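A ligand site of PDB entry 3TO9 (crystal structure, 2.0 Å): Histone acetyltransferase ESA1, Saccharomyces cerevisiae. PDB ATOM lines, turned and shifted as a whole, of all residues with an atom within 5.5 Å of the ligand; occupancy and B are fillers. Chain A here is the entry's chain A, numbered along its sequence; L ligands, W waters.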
ATOM      1  N   TRP A  21       6.021  -0.192 -12.235  1.00  0.00           N
ATOM      2  CA  TRP A  21       7.085  -0.226 -11.236  1.00  0.00           C
ATOM      3  C   TRP A  21       6.514  -0.749  -9.926  1.00  0.00           C
ATOM      4  O   TRP A  21       7.198  -1.432  -9.146  1.00  0.00           O
ATOM      5  CB  TRP A  21       7.682   1.163 -11.004  1.00  0.00           C
ATOM      6  CG  TRP A  21       8.277   1.825 -12.235  1.00  0.00           C
ATOM      7  CD1 TRP A  21       8.393   1.294 -13.496  1.00  0.00           C
ATOM      8  CD2 TRP A  21       8.839   3.141 -12.299  1.00  0.00           C
ATOM      9  NE1 TRP A  21       8.997   2.212 -14.344  1.00  0.00           N
ATOM     10  CE2 TRP A  21       9.261   3.354 -13.628  1.00  0.00           C
ATOM     11  CE3 TRP A  21       8.998   4.174 -11.362  1.00  0.00           C
ATOM     12  CZ2 TRP A  21       9.869   4.543 -14.036  1.00  0.00           C
ATOM     13  CZ3 TRP A  21       9.600   5.353 -11.764  1.00  0.00           C
ATOM     14  CH2 TRP A  21      10.026   5.526 -13.090  1.00  0.00           C
ATOM     15  N   PHE A  99       3.662   3.953 -11.031  1.00  0.00           N
ATOM     16  CA  PHE A  99       5.026   4.469 -11.089  1.00  0.00           C
ATOM     17  C   PHE A  99       5.417   5.246  -9.834  1.00  0.00           C
ATOM     18  O   PHE A  99       6.419   5.969  -9.818  1.00  0.00           O
ATOM     19  CB  PHE A  99       5.206   5.295 -12.367  1.00  0.00           C
ATOM     20  CG  PHE A  99       4.699   4.579 -13.583  1.00  0.00           C
ATOM     21  CD1 PHE A  99       5.355   3.450 -14.070  1.00  0.00           C
ATOM     22  CD2 PHE A  99       3.525   4.987 -14.220  1.00  0.00           C
ATOM     23  CE1 PHE A  99       4.882   2.765 -15.172  1.00  0.00           C
ATOM     24  CE2 PHE A  99       3.044   4.302 -15.315  1.00  0.00           C
ATOM     25  CZ  PHE A  99       3.727   3.186 -15.801  1.00  0.00           C
ATOM     26  N   LEU A 100       4.646   5.028  -8.773  1.00  0.00           N
ATOM     27  CA  LEU A 100       4.874   5.649  -7.469  1.00  0.00           C
ATOM     28  C   LEU A 100       4.820   4.604  -6.363  1.00  0.00           C
ATOM     29  O   LEU A 100       3.948   3.725  -6.348  1.00  0.00           O
ATOM     30  CB  LEU A 100       3.765   6.655  -7.193  1.00  0.00           C
ATOM     31  CG  LEU A 100       3.675   7.846  -8.138  1.00  0.00           C
ATOM     32  CD1 LEU A 100       2.358   8.565  -7.914  1.00  0.00           C
ATOM     33  CD2 LEU A 100       4.840   8.765  -7.854  1.00  0.00           C
ATOM     34  N   ALA A 144       1.564  18.495  -5.694  1.00  0.00           N
ATOM     35  CA  ALA A 144       1.286  17.330  -4.842  1.00  0.00           C
ATOM     36  C   ALA A 144       2.066  16.131  -5.375  1.00  0.00           C
ATOM     37  O   ALA A 144       2.952  15.612  -4.720  1.00  0.00           O
ATOM     38  CB  ALA A 144      -0.186  17.033  -4.803  1.00  0.00           C
ATOM     39  N   CYS A 145       1.754  15.718  -6.596  1.00  0.00           N
ATOM     40  CA  CYS A 145       2.555  14.713  -7.274  1.00  0.00           C
ATOM     41  C   CYS A 145       2.907  15.207  -8.679  1.00  0.00           C
ATOM     42  O   CYS A 145       2.211  16.032  -9.256  1.00  0.00           O
ATOM     43  CB  CYS A 145       1.808  13.398  -7.355  1.00  0.00           C
ATOM     44  SG  CYS A 145       2.900  12.054  -7.833  1.00  0.00           S
ATOM     45  N   ILE A 146       3.999  14.674  -9.232  1.00  0.00           N
ATOM     46  CA  ILE A 146       4.428  15.019 -10.575  1.00  0.00           C
ATOM     47  C   ILE A 146       4.890  13.745 -11.270  1.00  0.00           C
ATOM     48  O   ILE A 146       5.489  12.872 -10.640  1.00  0.00           O
ATOM     49  CB  ILE A 146       5.556  16.079 -10.549  1.00  0.00           C
ATOM     50  CG1 ILE A 146       5.991  16.460 -11.958  1.00  0.00           C
ATOM     51  CG2 ILE A 146       6.759  15.585  -9.736  1.00  0.00           C
ATOM     52  CD1 ILE A 146       6.796  17.747 -11.949  1.00  0.00           C
ATOM     53  N   LEU A 147       4.592  13.612 -12.550  1.00  0.00           N
ATOM     54  CA  LEU A 147       4.895  12.370 -13.270  1.00  0.00           C
ATOM     55  C   LEU A 147       5.105  12.632 -14.742  1.00  0.00           C
ATOM     56  O   LEU A 147       4.310  13.334 -15.359  1.00  0.00           O
ATOM     57  CB  LEU A 147       3.723  11.384 -13.147  1.00  0.00           C
ATOM     58  CG  LEU A 147       3.856  10.152 -14.055  1.00  0.00           C
ATOM     59  CD1 LEU A 147       4.817   9.157 -13.418  1.00  0.00           C
ATOM     60  CD2 LEU A 147       2.499   9.484 -14.343  1.00  0.00           C
ATOM     61  N   THR A 148       6.192  12.070 -15.286  1.00  0.00           N
ATOM     62  CA  THR A 148       6.354  11.915 -16.729  1.00  0.00           C
ATOM     63  C   THR A 148       6.151  10.423 -17.039  1.00  0.00           C
ATOM     64  O   THR A 148       6.761   9.563 -16.380  1.00  0.00           O
ATOM     65  CB  THR A 148       7.764  12.321 -17.175  1.00  0.00           C
ATOM     66  OG1 THR A 148       7.946  13.725 -16.954  1.00  0.00           O
ATOM     67  CG2 THR A 148       7.960  11.997 -18.649  1.00  0.00           C
ATOM     68  N   LEU A 149       5.295  10.108 -18.006  1.00  0.00           N
ATOM     69  CA  LEU A 149       5.070   8.693 -18.336  1.00  0.00           C
ATOM     70  C   LEU A 149       6.378   8.062 -18.743  1.00  0.00           C
ATOM     71  O   LEU A 149       7.196   8.703 -19.399  1.00  0.00           O
ATOM     72  CB  LEU A 149       4.018   8.539 -19.452  1.00  0.00           C
ATOM     73  CG  LEU A 149       2.651   9.131 -19.081  1.00  0.00           C
ATOM     74  CD1 LEU A 149       1.719   9.166 -20.293  1.00  0.00           C
ATOM     75  CD2 LEU A 149       2.010   8.348 -17.938  1.00  0.00           C
ATOM     76  N   TYR A 152       8.220   8.420 -21.971  1.00  0.00           N
ATOM     77  CA  TYR A 152       8.708   9.762 -22.296  1.00  0.00           C
ATOM     78  C   TYR A 152       9.737  10.298 -21.303  1.00  0.00           C
ATOM     79  O   TYR A 152      10.119  11.462 -21.397  1.00  0.00           O
ATOM     80  CB  TYR A 152       7.542  10.748 -22.398  1.00  0.00           C
ATOM     81  CG  TYR A 152       6.469  10.349 -23.387  1.00  0.00           C
ATOM     82  CD1 TYR A 152       6.758  10.223 -24.747  1.00  0.00           C
ATOM     83  CD2 TYR A 152       5.177  10.114 -22.979  1.00  0.00           C
ATOM     84  CE1 TYR A 152       5.762   9.867 -25.663  1.00  0.00           C
ATOM     85  CE2 TYR A 152       4.187   9.760 -23.874  1.00  0.00           C
ATOM     86  CZ  TYR A 152       4.482   9.637 -25.212  1.00  0.00           C
ATOM     87  OH  TYR A 152       3.484   9.282 -26.101  1.00  0.00           O
ATOM     88  N   GLN A 153      10.172   9.477 -20.358  1.00  0.00           N
ATOM     89  CA  GLN A 153      11.112   9.975 -19.347  1.00  0.00           C
ATOM     90  C   GLN A 153      12.496  10.289 -19.917  1.00  0.00           C
ATOM     91  O   GLN A 153      12.886   9.752 -20.949  1.00  0.00           O
ATOM     92  CB  GLN A 153      11.204   8.991 -18.165  1.00  0.00           C
ATOM     93  CG  GLN A 153       9.952   9.022 -17.295  1.00  0.00           C
ATOM     94  CD  GLN A 153       9.989   8.030 -16.143  1.00  0.00           C
ATOM     95  OE1 GLN A 153      10.962   7.278 -15.988  1.00  0.00           O
ATOM     96  NE2 GLN A 153       8.943   8.030 -15.331  1.00  0.00           N
ATOM     97  N   ARG A 154      13.225  11.177 -19.237  1.00  0.00           N
ATOM     98  CA  ARG A 154      14.580  11.539 -19.641  1.00  0.00           C
ATOM     99  C   ARG A 154      14.601  12.179 -21.032  1.00  0.00           C
ATOM    100  O   ARG A 154      15.515  11.945 -21.824  1.00  0.00           O
ATOM    101  CB  ARG A 154      15.536  10.327 -19.560  1.00  0.00           C
ATOM    102  CG  ARG A 154      15.584   9.695 -18.152  1.00  0.00           C
ATOM    103  CD  ARG A 154      16.603   8.552 -18.043  1.00  0.00           C
ATOM    104  NE  ARG A 154      17.987   9.028 -18.140  1.00  0.00           N
ATOM    105  CZ  ARG A 154      18.680   9.500 -17.105  1.00  0.00           C
ATOM    106  NH1 ARG A 154      19.926   9.905 -17.284  1.00  0.00           N
ATOM    107  NH2 ARG A 154      18.136   9.548 -15.898  1.00  0.00           N
ATOM    108  N   MET A 155      13.585  12.990 -21.306  1.00  0.00           N
ATOM    109  CA  MET A 155      13.524  13.782 -22.540  1.00  0.00           C
ATOM    110  C   MET A 155      13.393  15.269 -22.227  1.00  0.00           C
ATOM    111  O   MET A 155      13.291  16.097 -23.146  1.00  0.00           O
ATOM    112  CB  MET A 155      12.359  13.328 -23.425  1.00  0.00           C
ATOM    113  CG  MET A 155      12.544  11.930 -24.016  1.00  0.00           C
ATOM    114  SD  MET A 155      11.095  11.344 -24.924  1.00  0.00           S
ATOM    115  CE  MET A 155      11.077  12.474 -26.316  1.00  0.00           C
ATOM    116  N   GLY A 156      13.397  15.612 -20.948  1.00  0.00           N
ATOM    117  CA  GLY A 156      13.285  17.007 -20.531  1.00  0.00           C
ATOM    118  C   GLY A 156      11.883  17.446 -20.118  1.00  0.00           C
ATOM    119  O   GLY A 156      11.667  18.576 -19.727  1.00  0.00           O
ATOM    120  N   TYR A 157      10.921  16.531 -20.206  1.00  0.00           N
ATOM    121  CA  TYR A 157       9.532  16.904 -19.917  1.00  0.00           C
ATOM    122  C   TYR A 157       9.310  17.205 -18.443  1.00  0.00           C
ATOM    123  O   TYR A 157       8.551  18.112 -18.098  1.00  0.00           O
ATOM    124  CB  TYR A 157       8.589  15.795 -20.383  1.00  0.00           C
ATOM    125  CG  TYR A 157       8.566  15.607 -21.885  1.00  0.00           C
ATOM    126  CD1 TYR A 157       8.709  16.697 -22.740  1.00  0.00           C
ATOM    127  CD2 TYR A 157       8.407  14.345 -22.446  1.00  0.00           C
ATOM    128  CE1 TYR A 157       8.685  16.527 -24.122  1.00  0.00           C
ATOM    129  CE2 TYR A 157       8.390  14.166 -23.821  1.00  0.00           C
ATOM    130  CZ  TYR A 157       8.525  15.257 -24.655  1.00  0.00           C
ATOM    131  OH  TYR A 157       8.492  15.087 -26.017  1.00  0.00           O
ATOM    132  N   GLY A 158       9.929  16.420 -17.561  1.00  0.00           N
ATOM    133  CA  GLY A 158       9.796  16.646 -16.141  1.00  0.00           C
ATOM    134  C   GLY A 158      10.175  18.062 -15.760  1.00  0.00           C
ATOM    135  O   GLY A 158       9.487  18.702 -14.978  1.00  0.00           O
ATOM    136  N   LYS A 159      11.282  18.549 -16.314  1.00  0.00           N
ATOM    137  CA  LYS A 159      11.729  19.897 -15.996  1.00  0.00           C
ATOM    138  C   LYS A 159      10.717  20.957 -16.476  1.00  0.00           C
ATOM    139  O   LYS A 159      10.534  21.986 -15.829  1.00  0.00           O
ATOM    140  CB  LYS A 159      13.112  20.160 -16.584  1.00  0.00           C
ATOM    141  CG  LYS A 159      13.668  21.505 -16.175  1.00  0.00           C
ATOM    142  CD  LYS A 159      15.022  21.783 -16.794  1.00  0.00           C
ATOM    143  CE  LYS A 159      15.446  23.227 -16.512  1.00  0.00           C
ATOM    144  NZ  LYS A 159      16.888  23.449 -16.903  1.00  0.00           N
ATOM    145  N   LEU A 160      10.076  20.706 -17.605  1.00  0.00           N
ATOM    146  CA  LEU A 160       9.046  21.612 -18.099  1.00  0.00           C
ATOM    147  C   LEU A 160       7.848  21.634 -17.140  1.00  0.00           C
ATOM    148  O   LEU A 160       7.302  22.692 -16.849  1.00  0.00           O
ATOM    149  CB  LEU A 160       8.578  21.201 -19.493  1.00  0.00           C
ATOM    150  CG  LEU A 160       9.520  21.419 -20.693  1.00  0.00           C
ATOM    151  CD1 LEU A 160       8.873  20.836 -21.952  1.00  0.00           C
ATOM    152  CD2 LEU A 160       9.833  22.879 -20.921  1.00  0.00           C
ATOM    153  N   LEU A 161       7.448  20.462 -16.664  1.00  0.00           N
ATOM    154  CA  LEU A 161       6.366  20.378 -15.671  1.00  0.00           C
ATOM    155  C   LEU A 161       6.703  21.199 -14.414  1.00  0.00           C
ATOM    156  O   LEU A 161       5.866  21.957 -13.909  1.00  0.00           O
ATOM    157  CB  LEU A 161       6.111  18.904 -15.275  1.00  0.00           C
ATOM    158  CG  LEU A 161       5.453  17.982 -16.310  1.00  0.00           C
ATOM    159  CD1 LEU A 161       5.498  16.525 -15.835  1.00  0.00           C
ATOM    160  CD2 LEU A 161       4.015  18.416 -16.566  1.00  0.00           C
ATOM    161  N   LEU A 182       9.587  13.471  -0.947  1.00  0.00           N
ATOM    162  CA  LEU A 182       9.720  13.384  -2.389  1.00  0.00           C
ATOM    163  C   LEU A 182      10.450  12.100  -2.742  1.00  0.00           C
ATOM    164  O   LEU A 182      11.472  11.786  -2.120  1.00  0.00           O
ATOM    165  CB  LEU A 182      10.587  14.569  -2.825  1.00  0.00           C
ATOM    166  CG  LEU A 182      10.275  15.530  -3.983  1.00  0.00           C
ATOM    167  CD1 LEU A 182       8.830  15.529  -4.421  1.00  0.00           C
ATOM    168  CD2 LEU A 182      10.719  16.934  -3.577  1.00  0.00           C
ATOM    169  N   SER A 183       9.991  11.372  -3.756  1.00  0.00           N
ATOM    170  CA  SER A 183      10.728  10.212  -4.229  1.00  0.00           C
ATOM    171  C   SER A 183      12.145  10.644  -4.605  1.00  0.00           C
ATOM    172  O   SER A 183      12.409  11.828  -4.814  1.00  0.00           O
ATOM    173  CB  SER A 183      10.047   9.598  -5.454  1.00  0.00           C
ATOM    174  OG  SER A 183      10.205  10.429  -6.605  1.00  0.00           O
ATOM    175  N   LEU A 185      13.683  10.096  -7.444  1.00  0.00           N
ATOM    176  CA  LEU A 185      13.632  10.661  -8.785  1.00  0.00           C
ATOM    177  C   LEU A 185      13.067  12.074  -8.748  1.00  0.00           C
ATOM    178  O   LEU A 185      13.575  12.933  -9.407  1.00  0.00           O
ATOM    179  CB  LEU A 185      12.778   9.795  -9.707  1.00  0.00           C
ATOM    180  CG  LEU A 185      13.332   8.466 -10.152  1.00  0.00           C
ATOM    181  CD1 LEU A 185      12.332   7.739 -11.034  1.00  0.00           C
ATOM    182  CD2 LEU A 185      14.658   8.595 -10.857  1.00  0.00           C
ATOM    183  N   GLY A 186      12.061  12.298  -7.939  1.00  0.00           N
ATOM    184  CA  GLY A 186      11.460  13.621  -7.829  1.00  0.00           C
ATOM    185  C   GLY A 186      12.467  14.631  -7.283  1.00  0.00           C
ATOM    186  O   GLY A 186      12.671  15.694  -7.864  1.00  0.00           O
ATOM    187  N   LEU A 188      15.785  14.565  -7.117  1.00  0.00           N
ATOM    188  CA  LEU A 188      16.905  14.840  -8.026  1.00  0.00           C
ATOM    189  C   LEU A 188      16.484  15.760  -9.174  1.00  0.00           C
ATOM    190  O   LEU A 188      17.259  16.622  -9.611  1.00  0.00           O
ATOM    191  CB  LEU A 188      17.537  13.555  -8.548  1.00  0.00           C
ATOM    192  CG  LEU A 188      18.274  12.767  -7.447  1.00  0.00           C
ATOM    193  CD1 LEU A 188      18.871  11.487  -7.992  1.00  0.00           C
ATOM    194  CD2 LEU A 188      19.356  13.638  -6.824  1.00  0.00           C
ATOM    195  N   SER A 189      15.260  15.588  -9.660  1.00  0.00           N
ATOM    196  CA  SER A 189      14.753  16.465 -10.711  1.00  0.00           C
ATOM    197  C   SER A 189      14.611  17.893 -10.190  1.00  0.00           C
ATOM    198  O   SER A 189      15.033  18.833 -10.865  1.00  0.00           O
ATOM    199  CB  SER A 189      13.413  15.963 -11.270  1.00  0.00           C
ATOM    200  OG  SER A 189      13.648  14.885 -12.146  1.00  0.00           O
ATOM    201  N   LYS A 260      22.840  22.412 -24.646  1.00  0.00           N
ATOM    202  CA  LYS A 260      21.900  21.314 -24.780  1.00  0.00           C
ATOM    203  C   LYS A 260      20.643  21.705 -25.555  1.00  0.00           C
ATOM    204  O   LYS A 260      19.852  20.849 -25.942  1.00  0.00           O
ATOM    205  CB  LYS A 260      21.513  20.765 -23.401  1.00  0.00           C
ATOM    206  CG  LYS A 260      22.699  20.352 -22.558  1.00  0.00           C
ATOM    207  CD  LYS A 260      22.219  19.768 -21.240  1.00  0.00           C
ATOM    208  CE  LYS A 260      23.345  19.099 -20.506  1.00  0.00           C
ATOM    209  NZ  LYS A 260      22.840  18.407 -19.282  1.00  0.00           N
ATOM    210  N   ARG A 262      17.748  22.974 -24.779  1.00  0.00           N
ATOM    211  CA  ARG A 262      16.502  22.453 -24.203  1.00  0.00           C
ATOM    212  C   ARG A 262      15.355  23.470 -24.327  1.00  0.00           C
ATOM    213  O   ARG A 262      15.582  24.685 -24.305  1.00  0.00           O
ATOM    214  CB  ARG A 262      16.708  22.043 -22.742  1.00  0.00           C
ATOM    215  CG  ARG A 262      17.878  21.067 -22.471  1.00  0.00           C
ATOM    216  CD  ARG A 262      17.478  19.595 -22.608  1.00  0.00           C
ATOM    217  NE  ARG A 262      18.617  18.656 -22.504  1.00  0.00           N
ATOM    218  CZ  ARG A 262      19.032  18.108 -21.356  1.00  0.00           C
ATOM    219  NH1 ARG A 262      18.416  18.386 -20.216  1.00  0.00           N
ATOM    220  NH2 ARG A 262      20.065  17.272 -21.349  1.00  0.00           N
HETATM  221  N1  LIG L   1      18.991  13.330 -23.704  1.00  0.00           N
HETATM  222  C1  LIG L   1      19.563  12.701 -22.657  1.00  0.00           C
HETATM  223  N2  LIG L   1      19.167  12.921 -21.380  1.00  0.00           N
HETATM  224  C2  LIG L   1      18.158  13.797 -21.104  1.00  0.00           C
HETATM  225  C3  LIG L   1      17.522  14.480 -22.130  1.00  0.00           C
HETATM  226  C4  LIG L   1      17.987  14.210 -23.528  1.00  0.00           C
HETATM  227  N3  LIG L   1      17.416  14.837 -24.590  1.00  0.00           N
HETATM  228  N4  LIG L   1      16.573  15.269 -21.584  1.00  0.00           N
HETATM  229  C5  LIG L   1      16.618  15.077 -20.230  1.00  0.00           C
HETATM  230  N5  LIG L   1      17.587  14.181 -19.953  1.00  0.00           N
HETATM  231  C6  LIG L   1      18.002  13.675 -18.623  1.00  0.00           C
HETATM  232  C7  LIG L   1      18.283  14.804 -17.650  1.00  0.00           C
HETATM  233  O1  LIG L   1      19.570  15.391 -17.893  1.00  0.00           O
HETATM  234  C8  LIG L   1      18.160  14.079 -16.317  1.00  0.00           C
HETATM  235  O2  LIG L   1      19.299  13.236 -16.133  1.00  0.00           O
HETATM  236  P1  LIG L   1      20.036  12.992 -14.701  1.00  0.00           P
HETATM  237  O3  LIG L   1      21.087  11.911 -14.941  1.00  0.00           O
HETATM  238  O4  LIG L   1      18.989  12.539 -13.706  1.00  0.00           O
HETATM  239  O5  LIG L   1      20.603  14.397 -14.486  1.00  0.00           O
HETATM  240  C9  LIG L   1      17.006  13.103 -16.562  1.00  0.00           C
HETATM  241  O6  LIG L   1      16.989  12.880 -17.983  1.00  0.00           O
HETATM  242  C10 LIG L   1      15.624  13.589 -16.080  1.00  0.00           C
HETATM  243  O7  LIG L   1      15.243  14.911 -16.518  1.00  0.00           O
HETATM  244  P2  LIG L   1      13.803  15.116 -17.208  1.00  0.00           P
HETATM  245  O8  LIG L   1      13.822  14.302 -18.473  1.00  0.00           O
HETATM  246  O9  LIG L   1      13.469  16.573 -17.182  1.00  0.00           O
HETATM  247  O10 LIG L   1      12.765  14.425 -16.171  1.00  0.00           O
HETATM  248  P3  LIG L   1      11.687  13.268 -16.536  1.00  0.00           P
HETATM  249  O11 LIG L   1      12.412  11.971 -16.761  1.00  0.00           O
HETATM  250  O12 LIG L   1      10.779  13.796 -17.632  1.00  0.00           O
HETATM  251  O13 LIG L   1      10.788  13.245 -15.203  1.00  0.00           O
HETATM  252  C11 LIG L   1      10.258  12.580 -13.017  1.00  0.00           C
HETATM  253  C12 LIG L   1      11.343  13.217 -13.885  1.00  0.00           C
HETATM  254  C13 LIG L   1      10.586  12.669 -11.528  1.00  0.00           C
HETATM  255  C14 LIG L   1       8.957  13.329 -13.298  1.00  0.00           C
HETATM  256  C15 LIG L   1      10.171  11.122 -13.450  1.00  0.00           C
HETATM  257  O14 LIG L   1      11.341  10.451 -12.997  1.00  0.00           O
HETATM  258  C16 LIG L   1       8.967  10.414 -12.883  1.00  0.00           C
HETATM  259  O15 LIG L   1       7.777  10.605 -13.416  1.00  0.00           O
HETATM  260  N6  LIG L   1       9.138   9.560 -11.860  1.00  0.00           N
HETATM  261  C17 LIG L   1       8.110   8.755 -11.192  1.00  0.00           C
HETATM  262  C18 LIG L   1       7.116   9.690 -10.493  1.00  0.00           C
HETATM  263  C19 LIG L   1       7.694  10.326  -9.234  1.00  0.00           C
HETATM  264  O16 LIG L   1       8.503   9.711  -8.535  1.00  0.00           O
HETATM  265  N7  LIG L   1       7.277  11.552  -8.895  1.00  0.00           N
HETATM  266  C20 LIG L   1       7.720  12.279  -7.705  1.00  0.00           C
HETATM  267  C21 LIG L   1       6.564  13.155  -7.189  1.00  0.00           C
HETATM  268  S1  LIG L   1       5.262  12.188  -6.386  1.00  0.00           S
HETATM  269  O   HOH W   1      13.164  10.253 -14.932  1.00  0.00           O
HETATM  270  O   HOH W   2       7.074  11.728  -4.326  1.00  0.00           O
HETATM  271  O   HOH W   3      17.626  10.382 -12.186  1.00  0.00           O
HETATM  272  O   HOH W   4      16.758  16.185 -13.928  1.00  0.00           O
HETATM  273  O   HOH W   5       8.338   6.960  -8.260  1.00  0.00           O
HETATM  274  O   HOH W   6      11.140  13.609 -20.247  1.00  0.00           O
HETATM  275  O   HOH W   7      15.987  17.740 -17.835  1.00  0.00           O
HETATM  276  O   HOH W   8      17.411  14.296 -12.563  1.00  0.00           O
HETATM  277  O   HOH W   9      15.287  10.878 -13.916  1.00  0.00           O
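Merely in contact with the ligand: Leu 147, Ser 189, Leu 185, Leu 100, Phe 99, Trp 21, Tyr 157, Arg 262 and Gly 186.
Hydrophobic or aromatic side chains within 4 Å of the ligand: Trp 21, Leu 100, Ile 146, Leu 147 and Leu 185.
Within 4 Å of the ligand: Trp 21, Phe 99, Leu 100, Cys 145, Ile 146, Leu 147, Thr 148, Gln 153, Arg 154, Met 155, Gly 156, Tyr 157, Gly 158, Lys 159, Ser 183, Leu 185, Gly 186, Ser 189 and Arg 262.
The nearest printed residue that does not touch the ligand is Leu 182 (4.3 Å).
Water W5 lies within hydrogen-bond range of the backbone carbonyl oxygen (O) of Phe 99 (2.7 Å) and an oxygen (O16) of the ligand (2.8 Å).
Water W2 lies within hydrogen-bond range of a sulfur (S1) of the ligand and the backbone NH of Ser 183.
Water W7 bridges an oxygen (O9) of the ligand and the guanidinium group of Arg 262.
An oxygen (O16) of the ligand lies within hydrogen-bond range of the side-chain hydroxyl (OG) of Ser 183, 2.7 Å away.
The backbone NH (N) of Arg 154 lies within hydrogen-bond range of an oxygen (O11) of the ligand (2.7 Å).
O3 of the ligand is in salt-bridge range of NH1 of Arg 154, at 3.3 Å.
The backbone NH (N) of Gly 158 lies within hydrogen-bond range of an oxygen (O12) of the ligand (2.8 Å).
SG of Cys 145 lies close to S1 of the ligand (2.8 Å).
A nitrogen (N7) of the ligand is in hydrogen-bond range of the backbone carbonyl oxygen (O) of Ile 146.
N of Gly 156 sits at hydrogen-bond distance from O8 of the ligand, 2.8 Å away.
The backbone NH (N) of Thr 148 sits at hydrogen-bond distance from an oxygen (O15) of the ligand, 2.9 Å away.
O12 of the ligand is in hydrogen-bond range of OG1 of Thr 148 (2.9 Å).
The backbone NH (N) of Lys 159 is in hydrogen-bond range of an oxygen (O9) of the ligand, 3.1 Å away.
N of Met 155 lies within hydrogen-bond range of O8 of the ligand, at 3.1 Å.
NE2 of Gln 153 sits at hydrogen-bond distance from O15 of the ligand (3.4 Å).
N of Gly 186 sits at hydrogen-bond distance from OG of Ser 183 (3.0 Å).
The backbone NH (N) of Gly 158 is in hydrogen-bond range of the side-chain hydroxyl (OG1) of Thr 148.
The side-chain amide nitrogen of Gln 153 is in hydrogen-bond range of the backbone carbonyl oxygen of Thr 148, 2.9 Å away.
OG of Ser 189 is in hydrogen-bond range of O of Leu 185, at 3.4 Å.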
